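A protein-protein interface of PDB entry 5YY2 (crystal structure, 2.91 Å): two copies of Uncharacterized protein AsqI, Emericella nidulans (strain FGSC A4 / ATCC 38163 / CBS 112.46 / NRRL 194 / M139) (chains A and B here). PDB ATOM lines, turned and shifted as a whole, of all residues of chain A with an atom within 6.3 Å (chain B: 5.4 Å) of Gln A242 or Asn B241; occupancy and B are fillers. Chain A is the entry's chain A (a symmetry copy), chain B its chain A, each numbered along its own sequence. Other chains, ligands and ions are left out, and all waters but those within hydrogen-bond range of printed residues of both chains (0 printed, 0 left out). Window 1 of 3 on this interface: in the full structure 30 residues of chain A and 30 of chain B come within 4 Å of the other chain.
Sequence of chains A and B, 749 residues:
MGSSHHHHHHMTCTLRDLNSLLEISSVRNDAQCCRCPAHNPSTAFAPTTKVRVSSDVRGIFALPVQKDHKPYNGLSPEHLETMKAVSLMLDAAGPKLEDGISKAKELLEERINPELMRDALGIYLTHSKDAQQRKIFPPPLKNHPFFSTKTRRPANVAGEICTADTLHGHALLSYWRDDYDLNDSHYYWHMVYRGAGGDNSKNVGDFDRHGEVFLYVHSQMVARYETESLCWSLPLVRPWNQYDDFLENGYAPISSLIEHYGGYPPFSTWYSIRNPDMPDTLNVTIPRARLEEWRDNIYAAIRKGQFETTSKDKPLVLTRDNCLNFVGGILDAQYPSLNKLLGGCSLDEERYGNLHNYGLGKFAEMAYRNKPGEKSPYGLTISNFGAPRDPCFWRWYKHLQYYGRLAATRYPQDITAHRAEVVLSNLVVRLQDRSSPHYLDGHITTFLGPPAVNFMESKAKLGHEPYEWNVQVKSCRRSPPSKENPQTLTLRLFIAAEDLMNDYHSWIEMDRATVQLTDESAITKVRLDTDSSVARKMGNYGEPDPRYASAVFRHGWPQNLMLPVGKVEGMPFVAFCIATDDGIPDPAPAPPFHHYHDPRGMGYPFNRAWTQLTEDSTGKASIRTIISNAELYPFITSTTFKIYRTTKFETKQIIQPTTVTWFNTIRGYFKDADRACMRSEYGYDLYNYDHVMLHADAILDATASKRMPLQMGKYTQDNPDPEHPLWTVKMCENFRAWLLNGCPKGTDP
Of the 11 printed residues of chain B, 7 touch a printed residue of chain A.
Hydrophobic or aromatic side chains of chain B within 4 Å of the printed part of chain A: Pro B239 and Tyr B402.
Among the printed residues, 13 pairs touch across the chains.
Among the printed residues, Asp or Glu carboxylates within 4 Å of a Lys or Arg side-chain nitrogen of the other chain: Asp A244 with Arg B405.
The backbone carbonyl oxygen of Asn B241 lies within hydrogen-bond range of the guanidinium group of Arg B295, 3.3 Å away.
The backbone carbonyl oxygen of Asn A241 is in hydrogen-bond range of the guanidinium group of Arg A295 (3.3 Å).
The backbone carbonyl oxygen of Pro A239 sits at hydrogen-bond distance from the guanidinium group of Arg A395 (3.4 Å).
The side-chain carboxylate (OD2) of Asp A244 lies within salt-bridge range of the guanidinium group (NH1) of Arg B405, 3.1 Å away.
ND2 of Asn A241 lies close to NE2 of Gln B242 (2.9 Å).
The side-chain amide nitrogen (ND2) of Asn B241 sits close to the side-chain amide nitrogen (NE2) of Gln A242 (2.9 Å).
Among the printed residues, merely in contact across the chains: Gln A242 with Tyr B402, Tyr A402 with Gln B242, Arg A295 with Tyr B402, Tyr A402 with Arg B295, Gln A242 with Lys B398, Asn A241 with Tyr B402, Tyr A402 with Asn B241, Gln A242 with Pro B239, Pro A239 with Gln B242 and Gln A242 with Arg B405.
Of chain B, only Pro B239, Asn B241, Lys B398, Tyr B402 and Arg B405 come within 4 Å of Gln A242.
Of chain A, only Gln A242 (2.9 Å) and Tyr A402 (3.9 Å) come within 4 Å of Asn B241.
Printed residues of chain A within 4 Å of Tyr B402: Asn A241 (3.9 Å), Gln A242 (3.0 Å) and Arg A295 (3.5 Å).
Of the printed residues of chain B, Tyr A402 touches Asn B241, Gln B242 and Arg B295.
Trp B240 touches none of the printed residues of chain A.
The nearest printed residue of chain B that does not touch Gln A242 is His B399 (5.6 Å).
The nearest residue of chain A that does not touch Asn B241 is Asn A241 (5.0 Å).
Pro A239 touches Gln B242, and with the chains exchanged Gln A242 touches Pro B239.
Asn A241 touches Tyr B402, and with the chains exchanged Tyr A402 touches Asn B241.
Gln A242 touches Tyr B402, and with the chains exchanged Tyr A402 touches Gln B242.
Arg A295 touches Tyr B402, and with the chains exchanged Tyr A402 touches Arg B295.
Of the 13 pairs that touch across the chains among the printed residues, 10 have their exchanged pair printed and touching as well.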
ATOM      1  N   PRO A 239     -15.451  14.119 -19.430  1.00  0.00           N
ATOM      2  CA  PRO A 239     -16.521  14.772 -18.700  1.00  0.00           C
ATOM      3  C   PRO A 239     -15.978  15.808 -17.739  1.00  0.00           C
ATOM      4  O   PRO A 239     -14.847  15.699 -17.304  1.00  0.00           O
ATOM      5  CB  PRO A 239     -17.171  13.620 -17.961  1.00  0.00           C
ATOM      6  CG  PRO A 239     -16.116  12.632 -17.834  1.00  0.00           C
ATOM      7  CD  PRO A 239     -15.314  12.713 -19.047  1.00  0.00           C
ATOM      8  N   TRP A 240     -16.787  16.812 -17.438  1.00  0.00           N
ATOM      9  CA  TRP A 240     -16.465  17.827 -16.460  1.00  0.00           C
ATOM     10  C   TRP A 240     -16.777  17.298 -15.080  1.00  0.00           C
ATOM     11  O   TRP A 240     -17.633  17.812 -14.395  1.00  0.00           O
ATOM     12  CB  TRP A 240     -17.274  19.079 -16.739  1.00  0.00           C
ATOM     13  CG  TRP A 240     -16.850  20.289 -16.013  1.00  0.00           C
ATOM     14  CD1 TRP A 240     -17.469  20.862 -14.950  1.00  0.00           C
ATOM     15  CD2 TRP A 240     -15.725  21.105 -16.309  1.00  0.00           C
ATOM     16  NE1 TRP A 240     -16.793  21.981 -14.555  1.00  0.00           N
ATOM     17  CE2 TRP A 240     -15.715  22.154 -15.376  1.00  0.00           C
ATOM     18  CE3 TRP A 240     -14.721  21.058 -17.277  1.00  0.00           C
ATOM     19  CZ2 TRP A 240     -14.748  23.140 -15.383  1.00  0.00           C
ATOM     20  CZ3 TRP A 240     -13.759  22.042 -17.275  1.00  0.00           C
ATOM     21  CH2 TRP A 240     -13.778  23.063 -16.333  1.00  0.00           C
ATOM     22  N   ASN A 241     -16.087  16.250 -14.677  1.00  0.00           N
ATOM     23  CA  ASN A 241     -16.409  15.607 -13.424  1.00  0.00           C
ATOM     24  C   ASN A 241     -15.559  16.136 -12.304  1.00  0.00           C
ATOM     25  O   ASN A 241     -15.949  16.102 -11.138  1.00  0.00           O
ATOM     26  CB  ASN A 241     -16.245  14.100 -13.535  1.00  0.00           C
ATOM     27  CG  ASN A 241     -17.449  13.445 -14.128  1.00  0.00           C
ATOM     28  OD1 ASN A 241     -18.548  13.977 -14.047  1.00  0.00           O
ATOM     29  ND2 ASN A 241     -17.259  12.295 -14.741  1.00  0.00           N
ATOM     30  N   GLN A 242     -14.392  16.634 -12.673  1.00  0.00           N
ATOM     31  CA  GLN A 242     -13.522  17.299 -11.734  1.00  0.00           C
ATOM     32  C   GLN A 242     -13.659  18.785 -12.011  1.00  0.00           C
ATOM     33  O   GLN A 242     -13.498  19.229 -13.113  1.00  0.00           O
ATOM     34  CB  GLN A 242     -12.096  16.779 -11.876  1.00  0.00           C
ATOM     35  CG  GLN A 242     -12.015  15.258 -11.691  1.00  0.00           C
ATOM     36  CD  GLN A 242     -10.617  14.683 -11.799  1.00  0.00           C
ATOM     37  OE1 GLN A 242      -9.708  15.324 -12.287  1.00  0.00           O
ATOM     38  NE2 GLN A 242     -10.450  13.463 -11.353  1.00  0.00           N
ATOM     39  N   TYR A 243     -14.034  19.553 -11.013  1.00  0.00           N
ATOM     40  CA  TYR A 243     -14.381  20.941 -11.257  1.00  0.00           C
ATOM     41  C   TYR A 243     -13.172  21.872 -11.255  1.00  0.00           C
ATOM     42  O   TYR A 243     -13.308  23.069 -11.422  1.00  0.00           O
ATOM     43  CB  TYR A 243     -15.377  21.431 -10.215  1.00  0.00           C
ATOM     44  CG  TYR A 243     -16.769  20.861 -10.310  1.00  0.00           C
ATOM     45  CD1 TYR A 243     -17.135  20.013 -11.337  1.00  0.00           C
ATOM     46  CD2 TYR A 243     -17.724  21.191  -9.374  1.00  0.00           C
ATOM     47  CE1 TYR A 243     -18.415  19.501 -11.416  1.00  0.00           C
ATOM     48  CE2 TYR A 243     -18.983  20.689  -9.447  1.00  0.00           C
ATOM     49  CZ  TYR A 243     -19.327  19.849 -10.465  1.00  0.00           C
ATOM     50  OH  TYR A 243     -20.603  19.358 -10.511  1.00  0.00           O
ATOM     51  N   ASP A 244     -11.990  21.320 -11.051  1.00  0.00           N
ATOM     52  CA  ASP A 244     -10.777  22.100 -11.068  1.00  0.00           C
ATOM     53  C   ASP A 244     -10.022  21.797 -12.356  1.00  0.00           C
ATOM     54  O   ASP A 244      -8.809  21.959 -12.461  1.00  0.00           O
ATOM     55  CB  ASP A 244      -9.943  21.791  -9.832  1.00  0.00           C
ATOM     56  CG  ASP A 244      -9.674  20.321  -9.663  1.00  0.00           C
ATOM     57  OD1 ASP A 244     -10.075  19.533 -10.533  1.00  0.00           O
ATOM     58  OD2 ASP A 244      -9.045  19.951  -8.662  1.00  0.00           O
ATOM     59  N   ASP A 245     -10.775  21.339 -13.337  1.00  0.00           N
ATOM     60  CA  ASP A 245     -10.222  20.871 -14.577  1.00  0.00           C
ATOM     61  C   ASP A 245      -9.968  22.065 -15.471  1.00  0.00           C
ATOM     62  O   ASP A 245     -10.534  23.128 -15.276  1.00  0.00           O
ATOM     63  CB  ASP A 245     -11.175  19.875 -15.237  1.00  0.00           C
ATOM     64  CG  ASP A 245     -10.464  18.840 -16.072  1.00  0.00           C
ATOM     65  OD1 ASP A 245      -9.276  19.040 -16.375  1.00  0.00           O
ATOM     66  OD2 ASP A 245     -11.104  17.830 -16.433  1.00  0.00           O
ATOM     67  N   PHE A 246      -9.096  21.882 -16.449  1.00  0.00           N
ATOM     68  CA  PHE A 246      -8.792  22.910 -17.415  1.00  0.00           C
ATOM     69  C   PHE A 246      -9.636  22.739 -18.666  1.00  0.00           C
ATOM     70  O   PHE A 246     -10.014  21.633 -19.023  1.00  0.00           O
ATOM     71  CB  PHE A 246      -7.327  22.859 -17.803  1.00  0.00           C
ATOM     72  CG  PHE A 246      -6.389  23.107 -16.676  1.00  0.00           C
ATOM     73  CD1 PHE A 246      -6.134  24.390 -16.251  1.00  0.00           C
ATOM     74  CD2 PHE A 246      -5.738  22.066 -16.066  1.00  0.00           C
ATOM     75  CE1 PHE A 246      -5.269  24.627 -15.226  1.00  0.00           C
ATOM     76  CE2 PHE A 246      -4.874  22.295 -15.048  1.00  0.00           C
ATOM     77  CZ  PHE A 246      -4.636  23.581 -14.623  1.00  0.00           C
ATOM     78  N   GLU A 292     -19.216  21.946  -5.631  1.00  0.00           N
ATOM     79  CA  GLU A 292     -18.637  20.642  -5.357  1.00  0.00           C
ATOM     80  C   GLU A 292     -19.370  19.944  -4.231  1.00  0.00           C
ATOM     81  O   GLU A 292     -19.383  18.723  -4.141  1.00  0.00           O
ATOM     82  CB  GLU A 292     -17.160  20.767  -5.000  1.00  0.00           C
ATOM     83  CG  GLU A 292     -16.287  21.297  -6.105  1.00  0.00           C
ATOM     84  CD  GLU A 292     -14.846  21.049  -5.821  1.00  0.00           C
ATOM     85  OE1 GLU A 292     -14.562  20.641  -4.689  1.00  0.00           O
ATOM     86  OE2 GLU A 292     -14.009  21.244  -6.716  1.00  0.00           O
ATOM     87  N   ARG A 295     -22.651  18.537  -5.707  1.00  0.00           N
ATOM     88  CA  ARG A 295     -22.273  17.376  -6.492  1.00  0.00           C
ATOM     89  C   ARG A 295     -22.114  16.159  -5.596  1.00  0.00           C
ATOM     90  O   ARG A 295     -22.779  15.151  -5.776  1.00  0.00           O
ATOM     91  CB  ARG A 295     -20.975  17.640  -7.249  1.00  0.00           C
ATOM     92  CG  ARG A 295     -20.416  16.430  -7.961  1.00  0.00           C
ATOM     93  CD  ARG A 295     -18.977  16.680  -8.390  1.00  0.00           C
ATOM     94  NE  ARG A 295     -18.062  16.576  -7.263  1.00  0.00           N
ATOM     95  CZ  ARG A 295     -16.836  17.078  -7.240  1.00  0.00           C
ATOM     96  NH1 ARG A 295     -16.365  17.744  -8.274  1.00  0.00           N
ATOM     97  NH2 ARG A 295     -16.083  16.923  -6.171  1.00  0.00           N
ATOM     98  N   ARG A 395     -19.013  19.396 -22.356  1.00  0.00           N
ATOM     99  CA  ARG A 395     -18.251  18.712 -21.343  1.00  0.00           C
ATOM    100  C   ARG A 395     -19.043  18.741 -20.082  1.00  0.00           C
ATOM    101  O   ARG A 395     -18.883  17.898 -19.225  1.00  0.00           O
ATOM    102  CB  ARG A 395     -16.914  19.356 -21.139  1.00  0.00           C
ATOM    103  CG  ARG A 395     -16.001  19.155 -22.273  1.00  0.00           C
ATOM    104  CD  ARG A 395     -14.621  19.479 -21.827  1.00  0.00           C
ATOM    105  NE  ARG A 395     -14.251  18.626 -20.722  1.00  0.00           N
ATOM    106  CZ  ARG A 395     -13.232  18.873 -19.928  1.00  0.00           C
ATOM    107  NH1 ARG A 395     -12.509  19.954 -20.129  1.00  0.00           N
ATOM    108  NH2 ARG A 395     -12.937  18.049 -18.946  1.00  0.00           N
ATOM    109  N   HIS A 399     -21.000  15.532 -17.870  1.00  0.00           N
ATOM    110  CA  HIS A 399     -21.052  15.385 -16.428  1.00  0.00           C
ATOM    111  C   HIS A 399     -22.473  15.119 -15.969  1.00  0.00           C
ATOM    112  O   HIS A 399     -22.711  14.316 -15.080  1.00  0.00           O
ATOM    113  CB  HIS A 399     -20.518  16.628 -15.746  1.00  0.00           C
ATOM    114  CG  HIS A 399     -20.671  16.606 -14.263  1.00  0.00           C
ATOM    115  ND1 HIS A 399     -20.144  15.609 -13.475  1.00  0.00           N
ATOM    116  CD2 HIS A 399     -21.304  17.454 -13.422  1.00  0.00           C
ATOM    117  CE1 HIS A 399     -20.445  15.844 -12.212  1.00  0.00           C
ATOM    118  NE2 HIS A 399     -21.148  16.959 -12.153  1.00  0.00           N
ATOM    119  N   TYR A 402     -23.262  11.612 -16.275  1.00  0.00           N
ATOM    120  CA  TYR A 402     -22.671  10.760 -15.254  1.00  0.00           C
ATOM    121  C   TYR A 402     -23.714  10.403 -14.202  1.00  0.00           C
ATOM    122  O   TYR A 402     -23.759   9.287 -13.722  1.00  0.00           O
ATOM    123  CB  TYR A 402     -21.471  11.451 -14.615  1.00  0.00           C
ATOM    124  CG  TYR A 402     -20.772  10.641 -13.559  1.00  0.00           C
ATOM    125  CD1 TYR A 402     -20.395   9.332 -13.793  1.00  0.00           C
ATOM    126  CD2 TYR A 402     -20.473  11.193 -12.333  1.00  0.00           C
ATOM    127  CE1 TYR A 402     -19.751   8.601 -12.831  1.00  0.00           C
ATOM    128  CE2 TYR A 402     -19.835  10.465 -11.373  1.00  0.00           C
ATOM    129  CZ  TYR A 402     -19.475   9.177 -11.625  1.00  0.00           C
ATOM    130  OH  TYR A 402     -18.836   8.467 -10.656  1.00  0.00           O
ATOM    131  N   PRO B 239      -9.252  10.683 -16.587  1.00  0.00           N
ATOM    132  CA  PRO B 239      -9.174   9.786 -15.450  1.00  0.00           C
ATOM    133  C   PRO B 239     -10.156   8.642 -15.585  1.00  0.00           C
ATOM    134  O   PRO B 239     -11.162   8.781 -16.253  1.00  0.00           O
ATOM    135  CB  PRO B 239      -9.533  10.689 -14.288  1.00  0.00           C
ATOM    136  CG  PRO B 239     -10.340  11.738 -14.883  1.00  0.00           C
ATOM    137  CD  PRO B 239      -9.793  11.989 -16.209  1.00  0.00           C
ATOM    138  N   TRP B 240      -9.837   7.517 -14.963  1.00  0.00           N
ATOM    139  CA  TRP B 240     -10.710   6.366 -14.902  1.00  0.00           C
ATOM    140  C   TRP B 240     -11.718   6.570 -13.797  1.00  0.00           C
ATOM    141  O   TRP B 240     -11.738   5.840 -12.831  1.00  0.00           O
ATOM    142  CB  TRP B 240      -9.890   5.116 -14.644  1.00  0.00           C
ATOM    143  CG  TRP B 240     -10.594   3.837 -14.842  1.00  0.00           C
ATOM    144  CD1 TRP B 240     -11.052   3.000 -13.878  1.00  0.00           C
ATOM    145  CD2 TRP B 240     -10.901   3.223 -16.087  1.00  0.00           C
ATOM    146  NE1 TRP B 240     -11.637   1.903 -14.444  1.00  0.00           N
ATOM    147  CE2 TRP B 240     -11.557   2.015 -15.803  1.00  0.00           C
ATOM    148  CE3 TRP B 240     -10.683   3.571 -17.420  1.00  0.00           C
ATOM    149  CZ2 TRP B 240     -11.993   1.160 -16.796  1.00  0.00           C
ATOM    150  CZ3 TRP B 240     -11.124   2.716 -18.404  1.00  0.00           C
ATOM    151  CH2 TRP B 240     -11.774   1.530 -18.086  1.00  0.00           C
ATOM    152  N   ASN B 241     -12.550   7.582 -13.932  1.00  0.00           N
ATOM    153  CA  ASN B 241     -13.461   7.922 -12.864  1.00  0.00           C
ATOM    154  C   ASN B 241     -14.801   7.272 -13.061  1.00  0.00           C
ATOM    155  O   ASN B 241     -15.537   7.029 -12.107  1.00  0.00           O
ATOM    156  CB  ASN B 241     -13.624   9.429 -12.754  1.00  0.00           C
ATOM    157  CG  ASN B 241     -12.528  10.058 -11.958  1.00  0.00           C
ATOM    158  OD1 ASN B 241     -11.916   9.405 -11.123  1.00  0.00           O
ATOM    159  ND2 ASN B 241     -12.258  11.321 -12.213  1.00  0.00           N
ATOM    160  N   GLN B 242     -15.107   6.986 -14.315  1.00  0.00           N
ATOM    161  CA  GLN B 242     -16.295   6.243 -14.653  1.00  0.00           C
ATOM    162  C   GLN B 242     -15.832   4.838 -14.990  1.00  0.00           C
ATOM    163  O   GLN B 242     -14.975   4.644 -15.806  1.00  0.00           O
ATOM    164  CB  GLN B 242     -17.042   6.930 -15.791  1.00  0.00           C
ATOM    165  CG  GLN B 242     -17.401   8.383 -15.451  1.00  0.00           C
ATOM    166  CD  GLN B 242     -18.165   9.114 -16.536  1.00  0.00           C
ATOM    167  OE1 GLN B 242     -18.213   8.686 -17.672  1.00  0.00           O
ATOM    168  NE2 GLN B 242     -18.755  10.229 -16.187  1.00  0.00           N
ATOM    169  N   TYR B 243     -16.354   3.848 -14.300  1.00  0.00           N
ATOM    170  CA  TYR B 243     -15.810   2.509 -14.427  1.00  0.00           C
ATOM    171  C   TYR B 243     -16.395   1.731 -15.602  1.00  0.00           C
ATOM    172  O   TYR B 243     -16.054   0.585 -15.822  1.00  0.00           O
ATOM    173  CB  TYR B 243     -16.046   1.716 -13.149  1.00  0.00           C
ATOM    174  CG  TYR B 243     -15.241   2.141 -11.947  1.00  0.00           C
ATOM    175  CD1 TYR B 243     -14.285   3.134 -12.032  1.00  0.00           C
ATOM    176  CD2 TYR B 243     -15.431   1.529 -10.728  1.00  0.00           C
ATOM    177  CE1 TYR B 243     -13.551   3.512 -10.925  1.00  0.00           C
ATOM    178  CE2 TYR B 243     -14.713   1.898  -9.637  1.00  0.00           C
ATOM    179  CZ  TYR B 243     -13.775   2.884  -9.736  1.00  0.00           C
ATOM    180  OH  TYR B 243     -13.068   3.234  -8.619  1.00  0.00           O
ATOM    181  N   ARG B 295     -15.924   2.847  -4.188  1.00  0.00           N
ATOM    182  CA  ARG B 295     -15.622   4.176  -4.686  1.00  0.00           C
ATOM    183  C   ARG B 295     -16.574   5.198  -4.088  1.00  0.00           C
ATOM    184  O   ARG B 295     -16.158   6.144  -3.438  1.00  0.00           O
ATOM    185  CB  ARG B 295     -15.709   4.211  -6.209  1.00  0.00           C
ATOM    186  CG  ARG B 295     -15.572   5.592  -6.807  1.00  0.00           C
ATOM    187  CD  ARG B 295     -16.009   5.588  -8.264  1.00  0.00           C
ATOM    188  NE  ARG B 295     -17.459   5.561  -8.384  1.00  0.00           N
ATOM    189  CZ  ARG B 295     -18.118   5.199  -9.476  1.00  0.00           C
ATOM    190  NH1 ARG B 295     -17.467   4.809 -10.552  1.00  0.00           N
ATOM    191  NH2 ARG B 295     -19.435   5.214  -9.483  1.00  0.00           N
ATOM    192  N   TYR B 299     -15.859   8.171  -1.484  1.00  0.00           N
ATOM    193  CA  TYR B 299     -16.157   9.528  -1.906  1.00  0.00           C
ATOM    194  C   TYR B 299     -16.938  10.231  -0.816  1.00  0.00           C
ATOM    195  O   TYR B 299     -16.641  11.362  -0.432  1.00  0.00           O
ATOM    196  CB  TYR B 299     -16.990   9.574  -3.181  1.00  0.00           C
ATOM    197  CG  TYR B 299     -16.295   9.399  -4.514  1.00  0.00           C
ATOM    198  CD1 TYR B 299     -14.920   9.426  -4.646  1.00  0.00           C
ATOM    199  CD2 TYR B 299     -17.056   9.214  -5.657  1.00  0.00           C
ATOM    200  CE1 TYR B 299     -14.339   9.252  -5.896  1.00  0.00           C
ATOM    201  CE2 TYR B 299     -16.498   9.044  -6.873  1.00  0.00           C
ATOM    202  CZ  TYR B 299     -15.151   9.062  -7.004  1.00  0.00           C
ATOM    203  OH  TYR B 299     -14.655   8.881  -8.266  1.00  0.00           O
ATOM    204  N   LYS B 398      -4.693   8.183 -12.280  1.00  0.00           N
ATOM    205  CA  LYS B 398      -5.279   9.502 -12.378  1.00  0.00           C
ATOM    206  C   LYS B 398      -6.541   9.528 -11.535  1.00  0.00           C
ATOM    207  O   LYS B 398      -6.872  10.537 -10.926  1.00  0.00           O
ATOM    208  CB  LYS B 398      -5.585   9.861 -13.831  1.00  0.00           C
ATOM    209  CG  LYS B 398      -5.973  11.316 -14.064  1.00  0.00           C
ATOM    210  CD  LYS B 398      -4.841  12.248 -13.737  1.00  0.00           C
ATOM    211  CE  LYS B 398      -5.224  13.701 -13.920  1.00  0.00           C
ATOM    212  NZ  LYS B 398      -6.450  14.011 -13.141  1.00  0.00           N
ATOM    213  N   HIS B 399      -7.237   8.400 -11.494  1.00  0.00           N
ATOM    214  CA  HIS B 399      -8.402   8.247 -10.644  1.00  0.00           C
ATOM    215  C   HIS B 399      -8.001   8.261  -9.181  1.00  0.00           C
ATOM    216  O   HIS B 399      -8.679   8.839  -8.345  1.00  0.00           O
ATOM    217  CB  HIS B 399      -9.129   6.956 -10.963  1.00  0.00           C
ATOM    218  CG  HIS B 399     -10.256   6.663 -10.033  1.00  0.00           C
ATOM    219  ND1 HIS B 399     -11.305   7.530  -9.838  1.00  0.00           N
ATOM    220  CD2 HIS B 399     -10.496   5.599  -9.233  1.00  0.00           C
ATOM    221  CE1 HIS B 399     -12.143   7.015  -8.958  1.00  0.00           C
ATOM    222  NE2 HIS B 399     -11.674   5.842  -8.576  1.00  0.00           N
ATOM    223  N   TYR B 402      -7.680  11.653  -7.995  1.00  0.00           N
ATOM    224  CA  TYR B 402      -8.940  12.340  -7.756  1.00  0.00           C
ATOM    225  C   TYR B 402      -9.248  12.364  -6.263  1.00  0.00           C
ATOM    226  O   TYR B 402      -9.735  13.350  -5.743  1.00  0.00           O
ATOM    227  CB  TYR B 402     -10.068  11.667  -8.530  1.00  0.00           C
ATOM    228  CG  TYR B 402     -11.413  12.318  -8.370  1.00  0.00           C
ATOM    229  CD1 TYR B 402     -11.575  13.680  -8.541  1.00  0.00           C
ATOM    230  CD2 TYR B 402     -12.526  11.566  -8.064  1.00  0.00           C
ATOM    231  CE1 TYR B 402     -12.804  14.266  -8.401  1.00  0.00           C
ATOM    232  CE2 TYR B 402     -13.749  12.148  -7.920  1.00  0.00           C
ATOM    233  CZ  TYR B 402     -13.885  13.492  -8.091  1.00  0.00           C
ATOM    234  OH  TYR B 402     -15.115  14.057  -7.948  1.00  0.00           O
ATOM    235  N   ARG B 405      -7.387  15.041  -4.872  1.00  0.00           N
ATOM    236  CA  ARG B 405      -7.949  16.347  -5.175  1.00  0.00           C
ATOM    237  C   ARG B 405      -9.133  16.678  -4.309  1.00  0.00           C
ATOM    238  O   ARG B 405      -9.379  17.834  -3.999  1.00  0.00           O
ATOM    239  CB  ARG B 405      -8.383  16.424  -6.627  1.00  0.00           C
ATOM    240  CG  ARG B 405      -7.272  16.422  -7.590  1.00  0.00           C
ATOM    241  CD  ARG B 405      -7.806  16.451  -8.985  1.00  0.00           C
ATOM    242  NE  ARG B 405      -6.703  16.419  -9.918  1.00  0.00           N
ATOM    243  CZ  ARG B 405      -6.152  17.504 -10.430  1.00  0.00           C
ATOM    244  NH1 ARG B 405      -6.634  18.698 -10.120  1.00  0.00           N
ATOM    245  NH2 ARG B 405      -5.135  17.388 -11.257  1.00  0.00           N
